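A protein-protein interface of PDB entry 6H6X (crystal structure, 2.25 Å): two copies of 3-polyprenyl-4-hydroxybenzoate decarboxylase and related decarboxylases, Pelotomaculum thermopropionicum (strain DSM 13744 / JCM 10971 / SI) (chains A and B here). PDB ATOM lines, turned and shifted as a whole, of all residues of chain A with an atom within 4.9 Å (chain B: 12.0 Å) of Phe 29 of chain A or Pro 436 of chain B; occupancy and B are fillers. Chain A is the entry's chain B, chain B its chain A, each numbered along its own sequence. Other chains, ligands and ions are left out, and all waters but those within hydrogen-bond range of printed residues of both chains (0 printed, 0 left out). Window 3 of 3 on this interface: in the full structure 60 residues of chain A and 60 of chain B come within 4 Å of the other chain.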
ATOM      1  N   ASP A  26      -2.421  15.886   5.639  1.00  0.00           N
ATOM      2  CA  ASP A  26      -2.269  14.474   5.283  1.00  0.00           C
ATOM      3  C   ASP A  26      -1.351  14.362   4.030  1.00  0.00           C
ATOM      4  O   ASP A  26      -1.588  15.028   3.031  1.00  0.00           O
ATOM      5  CB  ASP A  26      -3.659  13.869   5.004  1.00  0.00           C
ATOM      6  CG  ASP A  26      -3.700  12.339   5.081  1.00  0.00           C
ATOM      7  OD1 ASP A  26      -2.711  11.623   4.789  1.00  0.00           O
ATOM      8  OD2 ASP A  26      -4.798  11.846   5.419  1.00  0.00           O
ATOM      9  N   PRO A  27      -0.315  13.502   4.066  1.00  0.00           N
ATOM     10  CA  PRO A  27       0.443  13.256   2.815  1.00  0.00           C
ATOM     11  C   PRO A  27      -0.376  12.610   1.681  1.00  0.00           C
ATOM     12  O   PRO A  27      -0.028  12.758   0.508  1.00  0.00           O
ATOM     13  CB  PRO A  27       1.537  12.300   3.283  1.00  0.00           C
ATOM     14  CG  PRO A  27       0.847  11.514   4.350  1.00  0.00           C
ATOM     15  CD  PRO A  27       0.134  12.591   5.123  1.00  0.00           C
ATOM     16  N   VAL A  28      -1.460  11.912   2.029  1.00  0.00           N
ATOM     17  CA  VAL A  28      -2.407  11.375   1.058  1.00  0.00           C
ATOM     18  C   VAL A  28      -3.302  12.513   0.592  1.00  0.00           C
ATOM     19  O   VAL A  28      -4.127  13.018   1.348  1.00  0.00           O
ATOM     20  CB  VAL A  28      -3.225  10.190   1.645  1.00  0.00           C
ATOM     21  CG1 VAL A  28      -4.231   9.619   0.633  1.00  0.00           C
ATOM     22  CG2 VAL A  28      -2.288   9.103   2.179  1.00  0.00           C
ATOM     23  N   PHE A  29      -3.042  12.976  -0.645  1.00  0.00           N
ATOM     24  CA  PHE A  29      -3.817  14.030  -1.364  1.00  0.00           C
ATOM     25  C   PHE A  29      -3.735  15.474  -0.887  1.00  0.00           C
ATOM     26  O   PHE A  29      -3.762  16.387  -1.712  1.00  0.00           O
ATOM     27  CB  PHE A  29      -5.289  13.666  -1.522  1.00  0.00           C
ATOM     28  CG  PHE A  29      -5.519  12.272  -2.033  1.00  0.00           C
ATOM     29  CD1 PHE A  29      -4.839  11.795  -3.138  1.00  0.00           C
ATOM     30  CD2 PHE A  29      -6.478  11.441  -1.423  1.00  0.00           C
ATOM     31  CE1 PHE A  29      -5.071  10.504  -3.613  1.00  0.00           C
ATOM     32  CE2 PHE A  29      -6.713  10.148  -1.889  1.00  0.00           C
ATOM     33  CZ  PHE A  29      -6.003   9.678  -2.992  1.00  0.00           C
ATOM     34  N   GLU A  30      -3.670  15.711   0.401  1.00  0.00           N
ATOM     35  CA  GLU A  30      -3.773  17.098   0.852  1.00  0.00           C
ATOM     36  C   GLU A  30      -2.550  17.937   0.518  1.00  0.00           C
ATOM     37  O   GLU A  30      -2.691  19.119   0.237  1.00  0.00           O
ATOM     38  CB  GLU A  30      -4.054  17.215   2.346  1.00  0.00           C
ATOM     39  CG  GLU A  30      -5.437  16.717   2.738  1.00  0.00           C
ATOM     40  CD  GLU A  30      -5.805  17.056   4.177  1.00  0.00           C
ATOM     41  OE1 GLU A  30      -4.895  17.350   4.988  1.00  0.00           O
ATOM     42  OE2 GLU A  30      -7.000  16.963   4.506  1.00  0.00           O
ATOM     43  N   ILE A  31      -1.361  17.357   0.579  1.00  0.00           N
ATOM     44  CA  ILE A  31      -0.146  18.109   0.215  1.00  0.00           C
ATOM     45  C   ILE A  31      -0.252  18.566  -1.225  1.00  0.00           C
ATOM     46  O   ILE A  31       0.047  19.727  -1.520  1.00  0.00           O
ATOM     47  CB  ILE A  31       1.155  17.301   0.436  1.00  0.00           C
ATOM     48  CG1 ILE A  31       1.443  17.242   1.944  1.00  0.00           C
ATOM     49  CG2 ILE A  31       2.336  17.942  -0.327  1.00  0.00           C
ATOM     50  CD1 ILE A  31       2.601  16.357   2.302  1.00  0.00           C
ATOM     51  N   ALA A  32      -0.728  17.679  -2.101  1.00  0.00           N
ATOM     52  CA  ALA A  32      -0.815  18.012  -3.519  1.00  0.00           C
ATOM     53  C   ALA A  32      -1.866  19.054  -3.740  1.00  0.00           C
ATOM     54  O   ALA A  32      -1.686  19.972  -4.539  1.00  0.00           O
ATOM     55  CB  ALA A  32      -1.123  16.783  -4.377  1.00  0.00           C
ATOM     56  N   ALA A  33      -2.989  18.899  -3.054  1.00  0.00           N
ATOM     57  CA  ALA A  33      -4.091  19.841  -3.188  1.00  0.00           C
ATOM     58  C   ALA A  33      -3.730  21.238  -2.693  1.00  0.00           C
ATOM     59  O   ALA A  33      -4.031  22.221  -3.336  1.00  0.00           O
ATOM     60  CB  ALA A  33      -5.287  19.315  -2.426  1.00  0.00           C
ATOM     61  N   THR A 121       0.999  10.822  -1.638  1.00  0.00           N
ATOM     62  CA  THR A 121       0.189  10.286  -2.722  1.00  0.00           C
ATOM     63  C   THR A 121      -0.426  11.526  -3.392  1.00  0.00           C
ATOM     64  O   THR A 121      -1.040  12.344  -2.752  1.00  0.00           O
ATOM     65  CB  THR A 121      -0.868   9.340  -2.136  1.00  0.00           C
ATOM     66  OG1 THR A 121      -0.215   8.405  -1.282  1.00  0.00           O
ATOM     67  CG2 THR A 121      -1.641   8.622  -3.185  1.00  0.00           C
ATOM     68  N   HIS A 122      -0.210  11.700  -4.686  1.00  0.00           N
ATOM     69  CA  HIS A 122      -0.434  13.002  -5.304  1.00  0.00           C
ATOM     70  C   HIS A 122      -1.847  13.197  -5.926  1.00  0.00           C
ATOM     71  O   HIS A 122      -2.526  14.128  -5.572  1.00  0.00           O
ATOM     72  CB  HIS A 122       0.667  13.302  -6.310  1.00  0.00           C
ATOM     73  CG  HIS A 122       2.014  13.453  -5.684  1.00  0.00           C
ATOM     74  ND1 HIS A 122       2.876  12.386  -5.507  1.00  0.00           N
ATOM     75  CD2 HIS A 122       2.630  14.535  -5.155  1.00  0.00           C
ATOM     76  CE1 HIS A 122       3.973  12.826  -4.922  1.00  0.00           C
ATOM     77  NE2 HIS A 122       3.861  14.127  -4.724  1.00  0.00           N
ATOM     78  N   HIS A 123      -2.226  12.345  -6.862  1.00  0.00           N
ATOM     79  CA  HIS A 123      -3.490  12.419  -7.587  1.00  0.00           C
ATOM     80  C   HIS A 123      -4.358  11.171  -7.307  1.00  0.00           C
ATOM     81  O   HIS A 123      -3.824  10.095  -6.980  1.00  0.00           O
ATOM     82  CB  HIS A 123      -3.213  12.532  -9.075  1.00  0.00           C
ATOM     83  CG  HIS A 123      -2.548  13.827  -9.463  1.00  0.00           C
ATOM     84  ND1 HIS A 123      -1.182  13.974  -9.591  1.00  0.00           N
ATOM     85  CD2 HIS A 123      -3.077  15.050  -9.723  1.00  0.00           C
ATOM     86  CE1 HIS A 123      -0.898  15.231  -9.888  1.00  0.00           C
ATOM     87  NE2 HIS A 123      -2.032  15.897  -9.998  1.00  0.00           N
ATOM     88  N   ALA A 124      -5.674  11.329  -7.505  1.00  0.00           N
ATOM     89  CA  ALA A 124      -6.721  10.295  -7.307  1.00  0.00           C
ATOM     90  C   ALA A 124      -6.400   8.938  -7.899  1.00  0.00           C
ATOM     91  O   ALA A 124      -6.434   7.944  -7.227  1.00  0.00           O
ATOM     92  CB  ALA A 124      -8.054  10.781  -7.907  1.00  0.00           C
ATOM     93  N   GLU B 431      -8.787  10.553 -19.698  1.00  0.00           N
ATOM     94  CA  GLU B 431      -9.242  11.139 -18.402  1.00  0.00           C
ATOM     95  C   GLU B 431      -8.214  12.120 -17.800  1.00  0.00           C
ATOM     96  O   GLU B 431      -7.010  11.790 -17.665  1.00  0.00           O
ATOM     97  CB  GLU B 431      -9.577  10.069 -17.341  1.00  0.00           C
ATOM     98  CG  GLU B 431     -10.077  10.666 -16.006  1.00  0.00           C
ATOM     99  CD  GLU B 431     -10.837   9.702 -15.107  1.00  0.00           C
ATOM    100  OE1 GLU B 431     -10.199   8.749 -14.588  1.00  0.00           O
ATOM    101  OE2 GLU B 431     -12.058   9.928 -14.887  1.00  0.00           O
ATOM    102  N   ARG B 432      -8.703  13.324 -17.461  1.00  0.00           N
ATOM    103  CA  ARG B 432      -7.893  14.362 -16.854  1.00  0.00           C
ATOM    104  C   ARG B 432      -7.559  13.925 -15.418  1.00  0.00           C
ATOM    105  O   ARG B 432      -8.387  13.318 -14.720  1.00  0.00           O
ATOM    106  CB  ARG B 432      -8.604  15.724 -16.887  1.00  0.00           C
ATOM    107  N   ILE B 433      -6.309  14.161 -15.014  1.00  0.00           N
ATOM    108  CA  ILE B 433      -5.877  13.870 -13.638  1.00  0.00           C
ATOM    109  C   ILE B 433      -6.580  14.875 -12.720  1.00  0.00           C
ATOM    110  O   ILE B 433      -6.974  15.955 -13.150  1.00  0.00           O
ATOM    111  CB  ILE B 433      -4.317  13.853 -13.455  1.00  0.00           C
ATOM    112  CG1 ILE B 433      -3.688  15.247 -13.681  1.00  0.00           C
ATOM    113  CG2 ILE B 433      -3.705  12.787 -14.353  1.00  0.00           C
ATOM    114  CD1 ILE B 433      -2.167  15.274 -13.628  1.00  0.00           C
ATOM    115  N   SER B 434      -6.752  14.483 -11.467  1.00  0.00           N
ATOM    116  CA  SER B 434      -7.273  15.370 -10.430  1.00  0.00           C
ATOM    117  C   SER B 434      -6.814  14.896  -9.042  1.00  0.00           C
ATOM    118  O   SER B 434      -6.317  13.758  -8.872  1.00  0.00           O
ATOM    119  CB  SER B 434      -8.818  15.466 -10.496  1.00  0.00           C
ATOM    120  OG  SER B 434      -9.443  14.203 -10.336  1.00  0.00           O
ATOM    121  N   ILE B 435      -7.013  15.780  -8.064  1.00  0.00           N
ATOM    122  CA  ILE B 435      -6.606  15.589  -6.673  1.00  0.00           C
ATOM    123  C   ILE B 435      -7.896  15.636  -5.833  1.00  0.00           C
ATOM    124  O   ILE B 435      -8.595  16.642  -5.884  1.00  0.00           O
ATOM    125  CB  ILE B 435      -5.635  16.727  -6.232  1.00  0.00           C
ATOM    126  CG1 ILE B 435      -4.483  16.929  -7.260  1.00  0.00           C
ATOM    127  CG2 ILE B 435      -5.053  16.421  -4.861  1.00  0.00           C
ATOM    128  CD1 ILE B 435      -3.800  18.295  -7.239  1.00  0.00           C
ATOM    129  N   PRO B 436      -8.246  14.541  -5.095  1.00  0.00           N
ATOM    130  CA  PRO B 436      -9.415  14.627  -4.181  1.00  0.00           C
ATOM    131  C   PRO B 436      -9.252  15.669  -3.040  1.00  0.00           C
ATOM    132  O   PRO B 436      -8.143  15.855  -2.491  1.00  0.00           O
ATOM    133  CB  PRO B 436      -9.561  13.188  -3.629  1.00  0.00           C
ATOM    134  CG  PRO B 436      -8.866  12.328  -4.630  1.00  0.00           C
ATOM    135  CD  PRO B 436      -7.712  13.165  -5.139  1.00  0.00           C
ATOM    136  N   GLY B 437     -10.358  16.349  -2.727  1.00  0.00           N
ATOM    137  CA  GLY B 437     -10.379  17.422  -1.733  1.00  0.00           C
ATOM    138  C   GLY B 437     -10.096  18.836  -2.239  1.00  0.00           C
ATOM    139  O   GLY B 437     -10.278  19.767  -1.482  1.00  0.00           O
ATOM    140  N   LEU B 438      -9.707  19.024  -3.511  1.00  0.00           N
ATOM    141  CA  LEU B 438      -9.210  20.321  -4.027  1.00  0.00           C
ATOM    142  C   LEU B 438     -10.271  21.441  -4.088  1.00  0.00           C
ATOM    143  O   LEU B 438      -9.923  22.612  -3.913  1.00  0.00           O
ATOM    144  CB  LEU B 438      -8.552  20.130  -5.422  1.00  0.00           C
ATOM    145  CG  LEU B 438      -7.732  21.166  -6.235  1.00  0.00           C
ATOM    146  CD1 LEU B 438      -8.373  21.507  -7.604  1.00  0.00           C
ATOM    147  CD2 LEU B 438      -7.314  22.435  -5.472  1.00  0.00           C
ATOM    148  N   ASP B 439     -11.536  21.091  -4.350  1.00  0.00           N
ATOM    149  CA  ASP B 439     -12.651  22.039  -4.170  1.00  0.00           C
ATOM    150  C   ASP B 439     -12.875  22.291  -2.660  1.00  0.00           C
ATOM    151  O   ASP B 439     -13.050  23.422  -2.213  1.00  0.00           O
ATOM    152  CB  ASP B 439     -13.923  21.506  -4.834  1.00  0.00           C
ATOM    153  N   LYS B 440     -12.792  21.223  -1.886  1.00  0.00           N
ATOM    154  CA  LYS B 440     -13.129  21.222  -0.463  1.00  0.00           C
ATOM    155  C   LYS B 440     -12.165  22.006   0.457  1.00  0.00           C
ATOM    156  O   LYS B 440     -12.571  22.390   1.561  1.00  0.00           O
ATOM    157  CB  LYS B 440     -13.256  19.772   0.072  1.00  0.00           C
ATOM    158  CG  LYS B 440     -14.146  18.819  -0.722  1.00  0.00           C
ATOM    159  CD  LYS B 440     -13.962  17.373  -0.268  1.00  0.00           C
ATOM    160  CE  LYS B 440     -14.426  16.394  -1.350  1.00  0.00           C
ATOM    161  NZ  LYS B 440     -14.361  14.971  -0.925  1.00  0.00           N
ATOM    162  N   ILE B 441     -10.915  22.255   0.029  1.00  0.00           N
ATOM    163  CA  ILE B 441      -9.826  22.697   0.934  1.00  0.00           C
ATOM    164  C   ILE B 441      -9.203  23.999   0.444  1.00  0.00           C
ATOM    165  O   ILE B 441      -8.948  24.155  -0.745  1.00  0.00           O
ATOM    166  CB  ILE B 441      -8.760  21.563   1.049  1.00  0.00           C
ATOM    167  CG1 ILE B 441      -9.362  20.301   1.708  1.00  0.00           C
ATOM    168  CG2 ILE B 441      -7.548  21.964   1.834  1.00  0.00           C
ATOM    169  CD1 ILE B 441     -10.049  20.481   3.067  1.00  0.00           C
ATOM    170  N   LYS B 442      -8.927  24.912   1.370  1.00  0.00           N
ATOM    171  CA  LYS B 442      -8.413  26.254   1.038  1.00  0.00           C
ATOM    172  C   LYS B 442      -7.066  26.478   1.723  1.00  0.00           C
ATOM    173  O   LYS B 442      -6.918  26.281   2.926  1.00  0.00           O
ATOM    174  CB  LYS B 442      -9.397  27.344   1.496  1.00  0.00           C
ATOM    175  CG  LYS B 442     -10.729  27.387   0.748  1.00  0.00           C
ATOM    176  CD  LYS B 442     -10.628  28.072  -0.621  1.00  0.00           C
ATOM    177  CE  LYS B 442     -11.823  27.715  -1.512  1.00  0.00           C
ATOM    178  NZ  LYS B 442     -11.683  26.406  -2.228  1.00  0.00           N
ATOM    179  N   LEU B 443      -6.081  26.902   0.942  1.00  0.00           N
ATOM    180  CA  LEU B 443      -4.726  27.143   1.432  1.00  0.00           C
ATOM    181  C   LEU B 443      -4.690  28.179   2.546  1.00  0.00           C
ATOM    182  O   LEU B 443      -3.930  28.000   3.498  1.00  0.00           O
ATOM    183  CB  LEU B 443      -3.836  27.616   0.271  1.00  0.00           C
ATOM    184  CG  LEU B 443      -2.348  27.900   0.553  1.00  0.00           C
ATOM    185  CD1 LEU B 443      -1.653  26.711   1.204  1.00  0.00           C
ATOM    186  CD2 LEU B 443      -1.670  28.303  -0.752  1.00  0.00           C
ATOM    187  N   TYR B 446      -4.887  26.972   6.236  1.00  0.00           N
ATOM    188  CA  TYR B 446      -3.770  26.162   6.759  1.00  0.00           C
ATOM    189  C   TYR B 446      -2.521  26.918   7.159  1.00  0.00           C
ATOM    190  O   TYR B 446      -1.725  26.401   7.965  1.00  0.00           O
ATOM    191  CB  TYR B 446      -3.387  25.063   5.765  1.00  0.00           C
ATOM    192  CG  TYR B 446      -4.362  23.937   5.741  1.00  0.00           C
ATOM    193  CD1 TYR B 446      -5.549  24.083   5.075  1.00  0.00           C
ATOM    194  CD2 TYR B 446      -4.134  22.753   6.442  1.00  0.00           C
ATOM    195  CE1 TYR B 446      -6.475  23.059   5.032  1.00  0.00           C
ATOM    196  CE2 TYR B 446      -5.076  21.722   6.424  1.00  0.00           C
ATOM    197  CZ  TYR B 446      -6.239  21.882   5.694  1.00  0.00           C
ATOM    198  OH  TYR B 446      -7.192  20.894   5.653  1.00  0.00           O
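The backbone NH of Ala 124 of chain A lies within hydrogen-bond range of the backbone carbonyl oxygen of Ser 434 of chain B (2.9 Å).
The backbone NH (N) of Phe 29 of chain A is in hydrogen-bond range of the backbone carbonyl oxygen (O) of Thr 121 of chain A, at 3.0 Å.
Printed residues of chain A that touch a printed residue of chain B: Phe 29, Ala 32, Ala 33, His 122, His 123 and Ala 124. Hydrophobic or aromatic side chains of chain B that line the printed part of chain A: Ile 433, Ile 435, Pro 436 and Leu 438. Among the printed residues, 11 pairs touch across the chains. Among the printed residues, no Asp or Glu carboxylate lies within 4 Å of a Lys or Arg side-chain nitrogen of the other chain.
Among the printed residues, merely in contact across the chains: Phe 29 of chain A with Ile 435 of chain B (3.4 Å), Phe 29 of chain A with Pro 436 of chain B (3.7 Å), Ala 32 of chain A with Ile 435 of chain B (3.8 Å), Ala 33 of chain A with Ile 435 of chain B (3.7 Å), Ala 33 of chain A with Leu 438 of chain B (3.9 Å), His 122 of chain A with Ile 435 of chain B (3.5 Å), His 123 of chain A with Ile 433 of chain B (3.7 Å), His 123 of chain A with Ser 434 of chain B (3.3 Å), His 123 of chain A with Ile 435 of chain B (3.4 Å) and Ala 124 of chain A with Pro 436 of chain B (3.6 Å).
No position is printed for both chains.
Phe 29 of chain A touches two residues of chain B. Printed residues of chain A within 4 Å of Pro 436 of chain B: Phe 29 and Ala 124. Pro 27 of chain A touches none of the printed residues of chain B. No residue of chain B comes within 4 Å of Glu 30 of chain A. Ile 31 of chain A touches none of the printed residues of chain B. Of chain B, only Ile 435 (3.8 Å) comes within 4 Å of Ala 32 of chain A. Thr 121 of chain A touches none of the printed residues of chain B. Of chain B, only Ser 434 (2.9 Å) and Pro 436 (3.6 Å) come within 4 Å of Ala 124 of chain A. Of the printed residues of chain A, Leu 438 of chain B touches Ala 33 (3.9 Å). Of the printed residues of chain A, Ile 435 of chain B touches Phe 29, Ala 32, Ala 33, His 122 and His 123. Printed residues of chain B within 4 Å of His 122 of chain A: Ile 435. Printed residues of chain A within 4 Å of Ser 434 of chain B: His 123 and Ala 124. Ile 441 of chain B touches none of the printed residues of chain A. Lys 442 of chain B touches none of the printed residues of chain A. The nearest printed residue of chain A that does not touch Pro 436 of chain B is His 123 of chain A (4.5 Å).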
